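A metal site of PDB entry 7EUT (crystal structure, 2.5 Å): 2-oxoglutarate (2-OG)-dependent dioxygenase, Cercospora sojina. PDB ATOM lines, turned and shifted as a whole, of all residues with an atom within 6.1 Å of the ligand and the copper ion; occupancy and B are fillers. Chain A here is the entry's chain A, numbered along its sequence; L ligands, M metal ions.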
ATOM      1  N   ARG A 140      30.258  30.631  15.426  1.00  0.00           N
ATOM      2  CA  ARG A 140      30.422  31.425  16.629  1.00  0.00           C
ATOM      3  C   ARG A 140      31.881  31.394  17.067  1.00  0.00           C
ATOM      4  O   ARG A 140      32.518  30.327  17.023  1.00  0.00           O
ATOM      5  CB  ARG A 140      29.522  30.909  17.761  1.00  0.00           C
ATOM      6  CG  ARG A 140      28.088  30.631  17.355  1.00  0.00           C
ATOM      7  CD  ARG A 140      27.298  30.084  18.524  1.00  0.00           C
ATOM      8  NE  ARG A 140      25.918  29.794  18.168  1.00  0.00           N
ATOM      9  CZ  ARG A 140      24.883  30.555  18.512  1.00  0.00           C
ATOM     10  NH1 ARG A 140      25.064  31.661  19.209  1.00  0.00           N
ATOM     11  NH2 ARG A 140      23.650  30.205  18.147  1.00  0.00           N
ATOM     12  N   THR A 164      28.493  35.601  19.163  1.00  0.00           N
ATOM     13  CA  THR A 164      28.836  35.092  20.501  1.00  0.00           C
ATOM     14  C   THR A 164      28.046  33.820  20.840  1.00  0.00           C
ATOM     15  O   THR A 164      27.211  33.425  20.066  1.00  0.00           O
ATOM     16  CB  THR A 164      28.597  36.117  21.609  1.00  0.00           C
ATOM     17  OG1 THR A 164      27.223  36.421  21.501  1.00  0.00           O
ATOM     18  CG2 THR A 164      29.433  37.372  21.474  1.00  0.00           C
ATOM     19  N   PRO A 165      28.359  33.180  21.942  1.00  0.00           N
ATOM     20  CA  PRO A 165      27.637  32.006  22.376  1.00  0.00           C
ATOM     21  C   PRO A 165      26.146  32.265  22.635  1.00  0.00           C
ATOM     22  O   PRO A 165      25.793  33.285  23.055  1.00  0.00           O
ATOM     23  CB  PRO A 165      28.264  31.731  23.730  1.00  0.00           C
ATOM     24  CG  PRO A 165      29.680  31.960  23.494  1.00  0.00           C
ATOM     25  CD  PRO A 165      29.692  33.077  22.494  1.00  0.00           C
ATOM     26  N   GLY A 166      25.329  31.264  22.326  1.00  0.00           N
ATOM     27  CA  GLY A 166      23.889  31.284  22.595  1.00  0.00           C
ATOM     28  C   GLY A 166      23.693  31.011  24.055  1.00  0.00           C
ATOM     29  O   GLY A 166      23.442  29.897  24.406  1.00  0.00           O
ATOM     30  N   ARG A 167      23.820  32.054  24.848  1.00  0.00           N
ATOM     31  CA  ARG A 167      23.804  31.930  26.307  1.00  0.00           C
ATOM     32  C   ARG A 167      22.395  32.101  26.882  1.00  0.00           C
ATOM     33  O   ARG A 167      22.163  32.912  27.784  1.00  0.00           O
ATOM     34  CB  ARG A 167      24.754  32.946  26.910  1.00  0.00           C
ATOM     35  CG  ARG A 167      25.473  32.469  28.160  1.00  0.00           C
ATOM     36  CD  ARG A 167      26.351  33.570  28.730  1.00  0.00           C
ATOM     37  NE  ARG A 167      27.764  33.226  28.684  1.00  0.00           N
ATOM     38  CZ  ARG A 167      28.709  33.879  29.356  1.00  0.00           C
ATOM     39  NH1 ARG A 167      28.389  34.906  30.128  1.00  0.00           N
ATOM     40  NH2 ARG A 167      29.979  33.504  29.263  1.00  0.00           N
ATOM     41  N   HIS A 170      16.867  27.639  24.885  1.00  0.00           N
ATOM     42  CA  HIS A 170      16.053  27.788  23.688  1.00  0.00           C
ATOM     43  C   HIS A 170      16.024  26.473  22.934  1.00  0.00           C
ATOM     44  O   HIS A 170      16.855  25.582  23.150  1.00  0.00           O
ATOM     45  CB  HIS A 170      16.597  28.898  22.773  1.00  0.00           C
ATOM     46  CG  HIS A 170      17.912  28.565  22.136  1.00  0.00           C
ATOM     47  ND1 HIS A 170      19.100  28.561  22.837  1.00  0.00           N
ATOM     48  CD2 HIS A 170      18.228  28.207  20.872  1.00  0.00           C
ATOM     49  CE1 HIS A 170      20.080  28.223  22.035  1.00  0.00           C
ATOM     50  NE2 HIS A 170      19.576  28.001  20.828  1.00  0.00           N
ATOM     51  N   VAL A 171      15.041  26.362  22.048  1.00  0.00           N
ATOM     52  CA  VAL A 171      15.022  25.362  20.987  1.00  0.00           C
ATOM     53  C   VAL A 171      14.918  26.122  19.669  1.00  0.00           C
ATOM     54  O   VAL A 171      14.038  26.966  19.500  1.00  0.00           O
ATOM     55  CB  VAL A 171      13.856  24.372  21.148  1.00  0.00           C
ATOM     56  CG1 VAL A 171      13.960  23.249  20.111  1.00  0.00           C
ATOM     57  CG2 VAL A 171      13.834  23.797  22.554  1.00  0.00           C
ATOM     58  N   ASP A 172      15.836  25.814  18.743  1.00  0.00           N
ATOM     59  CA  ASP A 172      15.976  26.644  17.542  1.00  0.00           C
ATOM     60  C   ASP A 172      14.705  26.695  16.708  1.00  0.00           C
ATOM     61  O   ASP A 172      14.520  27.669  15.962  1.00  0.00           O
ATOM     62  CB  ASP A 172      17.137  26.124  16.703  1.00  0.00           C
ATOM     63  CG  ASP A 172      18.487  26.451  17.312  1.00  0.00           C
ATOM     64  OD1 ASP A 172      18.629  26.315  18.551  1.00  0.00           O
ATOM     65  OD2 ASP A 172      19.402  26.847  16.568  1.00  0.00           O
ATOM     66  N   ASN A 203      20.523  20.064  14.653  1.00  0.00           N
ATOM     67  CA  ASN A 203      21.756  20.821  14.517  1.00  0.00           C
ATOM     68  C   ASN A 203      22.942  19.928  14.863  1.00  0.00           C
ATOM     69  O   ASN A 203      22.908  19.182  15.845  1.00  0.00           O
ATOM     70  CB  ASN A 203      21.754  22.048  15.422  1.00  0.00           C
ATOM     71  CG  ASN A 203      20.939  23.198  14.857  1.00  0.00           C
ATOM     72  OD1 ASN A 203      20.165  23.017  13.914  1.00  0.00           O
ATOM     73  ND2 ASN A 203      21.114  24.380  15.424  1.00  0.00           N
ATOM     74  N   VAL A 204      23.985  20.011  14.044  1.00  0.00           N
ATOM     75  CA  VAL A 204      25.228  19.287  14.277  1.00  0.00           C
ATOM     76  C   VAL A 204      26.261  20.316  14.741  1.00  0.00           C
ATOM     77  O   VAL A 204      26.687  21.176  13.956  1.00  0.00           O
ATOM     78  CB  VAL A 204      25.698  18.533  13.033  1.00  0.00           C
ATOM     79  CG1 VAL A 204      27.028  17.844  13.299  1.00  0.00           C
ATOM     80  CG2 VAL A 204      24.641  17.526  12.596  1.00  0.00           C
ATOM     81  N   TRP A 205      26.655  20.225  16.000  1.00  0.00           N
ATOM     82  CA  TRP A 205      27.488  21.220  16.658  1.00  0.00           C
ATOM     83  C   TRP A 205      28.892  20.663  16.855  1.00  0.00           C
ATOM     84  O   TRP A 205      29.078  19.668  17.564  1.00  0.00           O
ATOM     85  CB  TRP A 205      26.876  21.612  18.003  1.00  0.00           C
ATOM     86  CG  TRP A 205      27.501  22.793  18.680  1.00  0.00           C
ATOM     87  CD1 TRP A 205      27.055  24.075  18.664  1.00  0.00           C
ATOM     88  CD2 TRP A 205      28.671  22.785  19.518  1.00  0.00           C
ATOM     89  NE1 TRP A 205      27.876  24.876  19.419  1.00  0.00           N
ATOM     90  CE2 TRP A 205      28.880  24.103  19.948  1.00  0.00           C
ATOM     91  CE3 TRP A 205      29.564  21.790  19.922  1.00  0.00           C
ATOM     92  CZ2 TRP A 205      29.940  24.466  20.774  1.00  0.00           C
ATOM     93  CZ3 TRP A 205      30.623  22.139  20.747  1.00  0.00           C
ATOM     94  CH2 TRP A 205      30.799  23.468  21.162  1.00  0.00           C
ATOM     95  N   GLU A 214      33.170  28.052  27.721  1.00  0.00           N
ATOM     96  CA  GLU A 214      31.782  28.170  27.271  1.00  0.00           C
ATOM     97  C   GLU A 214      31.305  26.931  26.528  1.00  0.00           C
ATOM     98  O   GLU A 214      31.037  26.983  25.321  1.00  0.00           O
ATOM     99  CB  GLU A 214      31.619  29.410  26.382  1.00  0.00           C
ATOM    100  CG  GLU A 214      30.172  29.830  26.152  1.00  0.00           C
ATOM    101  CD  GLU A 214      29.741  30.982  27.045  1.00  0.00           C
ATOM    102  OE1 GLU A 214      30.616  31.754  27.488  1.00  0.00           O
ATOM    103  OE2 GLU A 214      28.519  31.107  27.300  1.00  0.00           O
ATOM    104  N   PRO A 215      31.174  25.791  27.213  1.00  0.00           N
ATOM    105  CA  PRO A 215      30.659  24.589  26.529  1.00  0.00           C
ATOM    106  C   PRO A 215      29.161  24.674  26.245  1.00  0.00           C
ATOM    107  O   PRO A 215      28.527  25.690  26.550  1.00  0.00           O
ATOM    108  CB  PRO A 215      30.973  23.455  27.512  1.00  0.00           C
ATOM    109  CG  PRO A 215      31.042  24.123  28.844  1.00  0.00           C
ATOM    110  CD  PRO A 215      31.553  25.512  28.605  1.00  0.00           C
ATOM    111  N   LEU A 216      28.597  23.628  25.659  1.00  0.00           N
ATOM    112  CA  LEU A 216      27.207  23.625  25.202  1.00  0.00           C
ATOM    113  C   LEU A 216      26.413  22.601  26.002  1.00  0.00           C
ATOM    114  O   LEU A 216      26.677  21.400  25.909  1.00  0.00           O
ATOM    115  CB  LEU A 216      27.129  23.317  23.707  1.00  0.00           C
ATOM    116  CG  LEU A 216      25.745  23.518  23.100  1.00  0.00           C
ATOM    117  CD1 LEU A 216      25.322  24.971  23.234  1.00  0.00           C
ATOM    118  CD2 LEU A 216      25.723  23.084  21.643  1.00  0.00           C
ATOM    119  N   MET A 250      11.030  30.098  17.519  1.00  0.00           N
ATOM    120  CA  MET A 250      11.768  29.269  18.454  1.00  0.00           C
ATOM    121  C   MET A 250      10.867  28.858  19.617  1.00  0.00           C
ATOM    122  O   MET A 250       9.762  29.367  19.797  1.00  0.00           O
ATOM    123  CB  MET A 250      12.980  30.012  19.000  1.00  0.00           C
ATOM    124  CG  MET A 250      14.122  30.221  18.029  1.00  0.00           C
ATOM    125  SD  MET A 250      15.592  30.778  18.922  1.00  0.00           S
ATOM    126  CE  MET A 250      16.880  30.337  17.772  1.00  0.00           C
ATOM    127  N   ILE A 278      21.737  17.658  18.042  1.00  0.00           N
ATOM    128  CA  ILE A 278      20.681  18.249  18.873  1.00  0.00           C
ATOM    129  C   ILE A 278      19.392  18.257  18.069  1.00  0.00           C
ATOM    130  O   ILE A 278      19.269  19.035  17.110  1.00  0.00           O
ATOM    131  CB  ILE A 278      21.043  19.654  19.360  1.00  0.00           C
ATOM    132  CG1 ILE A 278      22.452  19.679  19.958  1.00  0.00           C
ATOM    133  CG2 ILE A 278      20.015  20.144  20.375  1.00  0.00           C
ATOM    134  CD1 ILE A 278      22.797  20.994  20.622  1.00  0.00           C
ATOM    135  N   MET A 280      16.037  19.470  17.233  1.00  0.00           N
ATOM    136  CA  MET A 280      15.166  20.612  17.499  1.00  0.00           C
ATOM    137  C   MET A 280      13.700  20.258  17.326  1.00  0.00           C
ATOM    138  O   MET A 280      12.841  20.795  18.050  1.00  0.00           O
ATOM    139  CB  MET A 280      15.517  21.765  16.560  1.00  0.00           C
ATOM    140  CG  MET A 280      16.977  22.133  16.541  1.00  0.00           C
ATOM    141  SD  MET A 280      17.549  22.591  18.178  1.00  0.00           S
ATOM    142  CE  MET A 280      19.298  22.826  17.866  1.00  0.00           C
ATOM    143  N   HIS A 294      18.526  23.898  24.880  1.00  0.00           N
ATOM    144  CA  HIS A 294      19.976  23.900  24.978  1.00  0.00           C
ATOM    145  C   HIS A 294      20.441  25.334  25.188  1.00  0.00           C
ATOM    146  O   HIS A 294      19.720  26.291  24.901  1.00  0.00           O
ATOM    147  CB  HIS A 294      20.637  23.288  23.738  1.00  0.00           C
ATOM    148  CG  HIS A 294      20.181  23.903  22.450  1.00  0.00           C
ATOM    149  ND1 HIS A 294      18.920  23.701  21.938  1.00  0.00           N
ATOM    150  CD2 HIS A 294      20.826  24.706  21.569  1.00  0.00           C
ATOM    151  CE1 HIS A 294      18.792  24.364  20.800  1.00  0.00           C
ATOM    152  NE2 HIS A 294      19.937  24.976  20.553  1.00  0.00           N
ATOM    153  N   SER A 295      21.668  25.461  25.691  1.00  0.00           N
ATOM    154  CA  SER A 295      22.250  26.764  25.961  1.00  0.00           C
ATOM    155  C   SER A 295      23.734  26.595  26.258  1.00  0.00           C
ATOM    156  O   SER A 295      24.125  25.629  26.920  1.00  0.00           O
ATOM    157  CB  SER A 295      21.554  27.459  27.146  1.00  0.00           C
ATOM    158  OG  SER A 295      22.366  28.488  27.680  1.00  0.00           O
ATOM    159  N   SER A 296      24.530  27.530  25.763  1.00  0.00           N
ATOM    160  CA  SER A 296      25.916  27.619  26.205  1.00  0.00           C
ATOM    161  C   SER A 296      25.960  28.151  27.634  1.00  0.00           C
ATOM    162  O   SER A 296      25.070  28.877  28.077  1.00  0.00           O
ATOM    163  CB  SER A 296      26.719  28.526  25.276  1.00  0.00           C
ATOM    164  OG  SER A 296      26.262  29.869  25.364  1.00  0.00           O
ATOM    165  N   ARG A 307      35.980  30.106  22.679  1.00  0.00           N
ATOM    166  CA  ARG A 307      35.412  28.942  22.028  1.00  0.00           C
ATOM    167  C   ARG A 307      34.923  29.294  20.624  1.00  0.00           C
ATOM    168  O   ARG A 307      34.258  30.314  20.427  1.00  0.00           O
ATOM    169  CB  ARG A 307      34.250  28.385  22.857  1.00  0.00           C
ATOM    170  CG  ARG A 307      33.784  27.000  22.443  1.00  0.00           C
ATOM    171  CD  ARG A 307      32.423  27.038  21.764  1.00  0.00           C
ATOM    172  NE  ARG A 307      31.340  27.386  22.685  1.00  0.00           N
ATOM    173  CZ  ARG A 307      30.215  27.986  22.316  1.00  0.00           C
ATOM    174  NH1 ARG A 307      30.015  28.311  21.044  1.00  0.00           N
ATOM    175  NH2 ARG A 307      29.280  28.267  23.215  1.00  0.00           N
ATOM    176  N   SER A 309      33.058  27.475  17.097  1.00  0.00           N
ATOM    177  CA  SER A 309      32.253  26.327  16.724  1.00  0.00           C
ATOM    178  C   SER A 309      31.403  26.663  15.505  1.00  0.00           C
ATOM    179  O   SER A 309      31.178  27.832  15.191  1.00  0.00           O
ATOM    180  CB  SER A 309      31.349  25.867  17.874  1.00  0.00           C
ATOM    181  OG  SER A 309      30.337  26.828  18.127  1.00  0.00           O
ATOM    182  N   GLU A 311      27.530  25.274  14.043  1.00  0.00           N
ATOM    183  CA  GLU A 311      26.329  24.466  14.168  1.00  0.00           C
ATOM    184  C   GLU A 311      25.657  24.453  12.808  1.00  0.00           C
ATOM    185  O   GLU A 311      25.278  25.506  12.284  1.00  0.00           O
ATOM    186  CB  GLU A 311      25.393  25.018  15.251  1.00  0.00           C
ATOM    187  CG  GLU A 311      25.039  26.490  15.080  1.00  0.00           C
ATOM    188  CD  GLU A 311      24.965  27.241  16.385  1.00  0.00           C
ATOM    189  OE1 GLU A 311      24.018  28.037  16.554  1.00  0.00           O
ATOM    190  OE2 GLU A 311      25.858  27.055  17.243  1.00  0.00           O
HETATM  191  C1  LIG L   1      22.955  25.492  18.472  1.00  0.00           C
HETATM  192  C2  LIG L   1      23.278  26.526  19.544  1.00  0.00           C
HETATM  193  C3  LIG L   1      24.898  27.940  20.808  1.00  0.00           C
HETATM  194  C4  LIG L   1      26.402  28.054  21.057  1.00  0.00           C
HETATM  195  O1  LIG L   1      23.878  24.779  17.999  1.00  0.00           O
HETATM  196  O2  LIG L   1      21.764  25.353  18.074  1.00  0.00           O
HETATM  197  O3  LIG L   1      22.396  26.989  20.194  1.00  0.00           O
HETATM  198  O4  LIG L   1      26.833  28.882  21.900  1.00  0.00           O
HETATM  199  N1  LIG L   1      24.644  26.949  19.780  1.00  0.00           N
HETATM  200  O5  LIG L   1      27.204  27.334  20.422  1.00  0.00           O
HETATM  201 CU    CU M   1      20.534  26.702  19.306  1.00  0.00          CU
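NE1 of Trp 205 sits at hydrogen-bond distance from O5 of the ligand (2.7 Å).
OE2 of Glu 311 lies within hydrogen-bond range of N1 of the ligand (2.8 Å).
The guanidinium group of Arg 307 is in salt-bridge range of an oxygen (O4) of the ligand (2.8 Å).
The backbone NH of Gly 166 is in hydrogen-bond range of an oxygen (O4) of the ligand (2.8 Å).
The side-chain amide nitrogen (ND2) of Asn 203 lies close to an oxygen (O2) of the ligand (2.9 Å).
The guanidinium group of Arg 140 is in salt-bridge range of an oxygen (O5) of the ligand (3.6 Å).
OD2 of Asp 172 is in hydrogen-bond range of ND2 of Asn 203, at 3.2 Å.
N of Asp 172 lies within hydrogen-bond range of SD of Met 280.
OG of Ser 309 is in hydrogen-bond range of NE1 of Trp 205 (3.4 Å).
NH2 of Arg 140 lies within salt-bridge range of OE1 of Glu 311, at 2.7 Å.
O of Glu 214 lies within hydrogen-bond range of NE of Arg 307, at 2.7 Å.
The backbone carbonyl oxygen (O) of Gly 166 is in hydrogen-bond range of the backbone NH (N) of Ser 296 (2.9 Å).
The guanidinium group of Arg 140 lies within hydrogen-bond range of the backbone carbonyl oxygen of Thr 164.
OG of Ser 296 sits at hydrogen-bond distance from N of Arg 167.
Merely in contact with the ligand: Pro 165 (3.3 Å), Leu 216 (3.9 Å), Met 280 (3.5 Å), Ser 296 (3.4 Å) and Ser 309 (3.9 Å).
Hydrophobic or aromatic side chains within 4 Å of the ligand: Pro 165, His 170, Trp 205, Leu 216, Met 280 and His 294.
14 residues have an atom within 4 Å of the ligand: Arg 140, Pro 165, Gly 166, His 170, Asp 172, Asn 203, Trp 205, Leu 216, Met 280, His 294, Ser 296, Arg 307, Ser 309 and Glu 311.
The nearest printed residue that does not touch the ligand is Ile 278 (4.7 Å).
Three residues have an atom within 4 Å of the copper ion: His 170, Asp 172 and His 294.
The nearest printed residue that does not touch the copper ion is Met 280 (4.3 Å).
O3 of the ligand is bound to the copper ion (2.1 Å).
The copper ion is bound by the side-chain carboxylate (OD1) of Asp 172 (2.1 Å).
O2 of the ligand is bound to the copper ion (2.2 Å).
The copper ion is bound by a ring nitrogen (NE2) of His 294, 2.2 Å away.
The copper ion is bound by NE2 of His 170, at 2.2 Å.
The copper ion has five donor atoms within binding distance.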
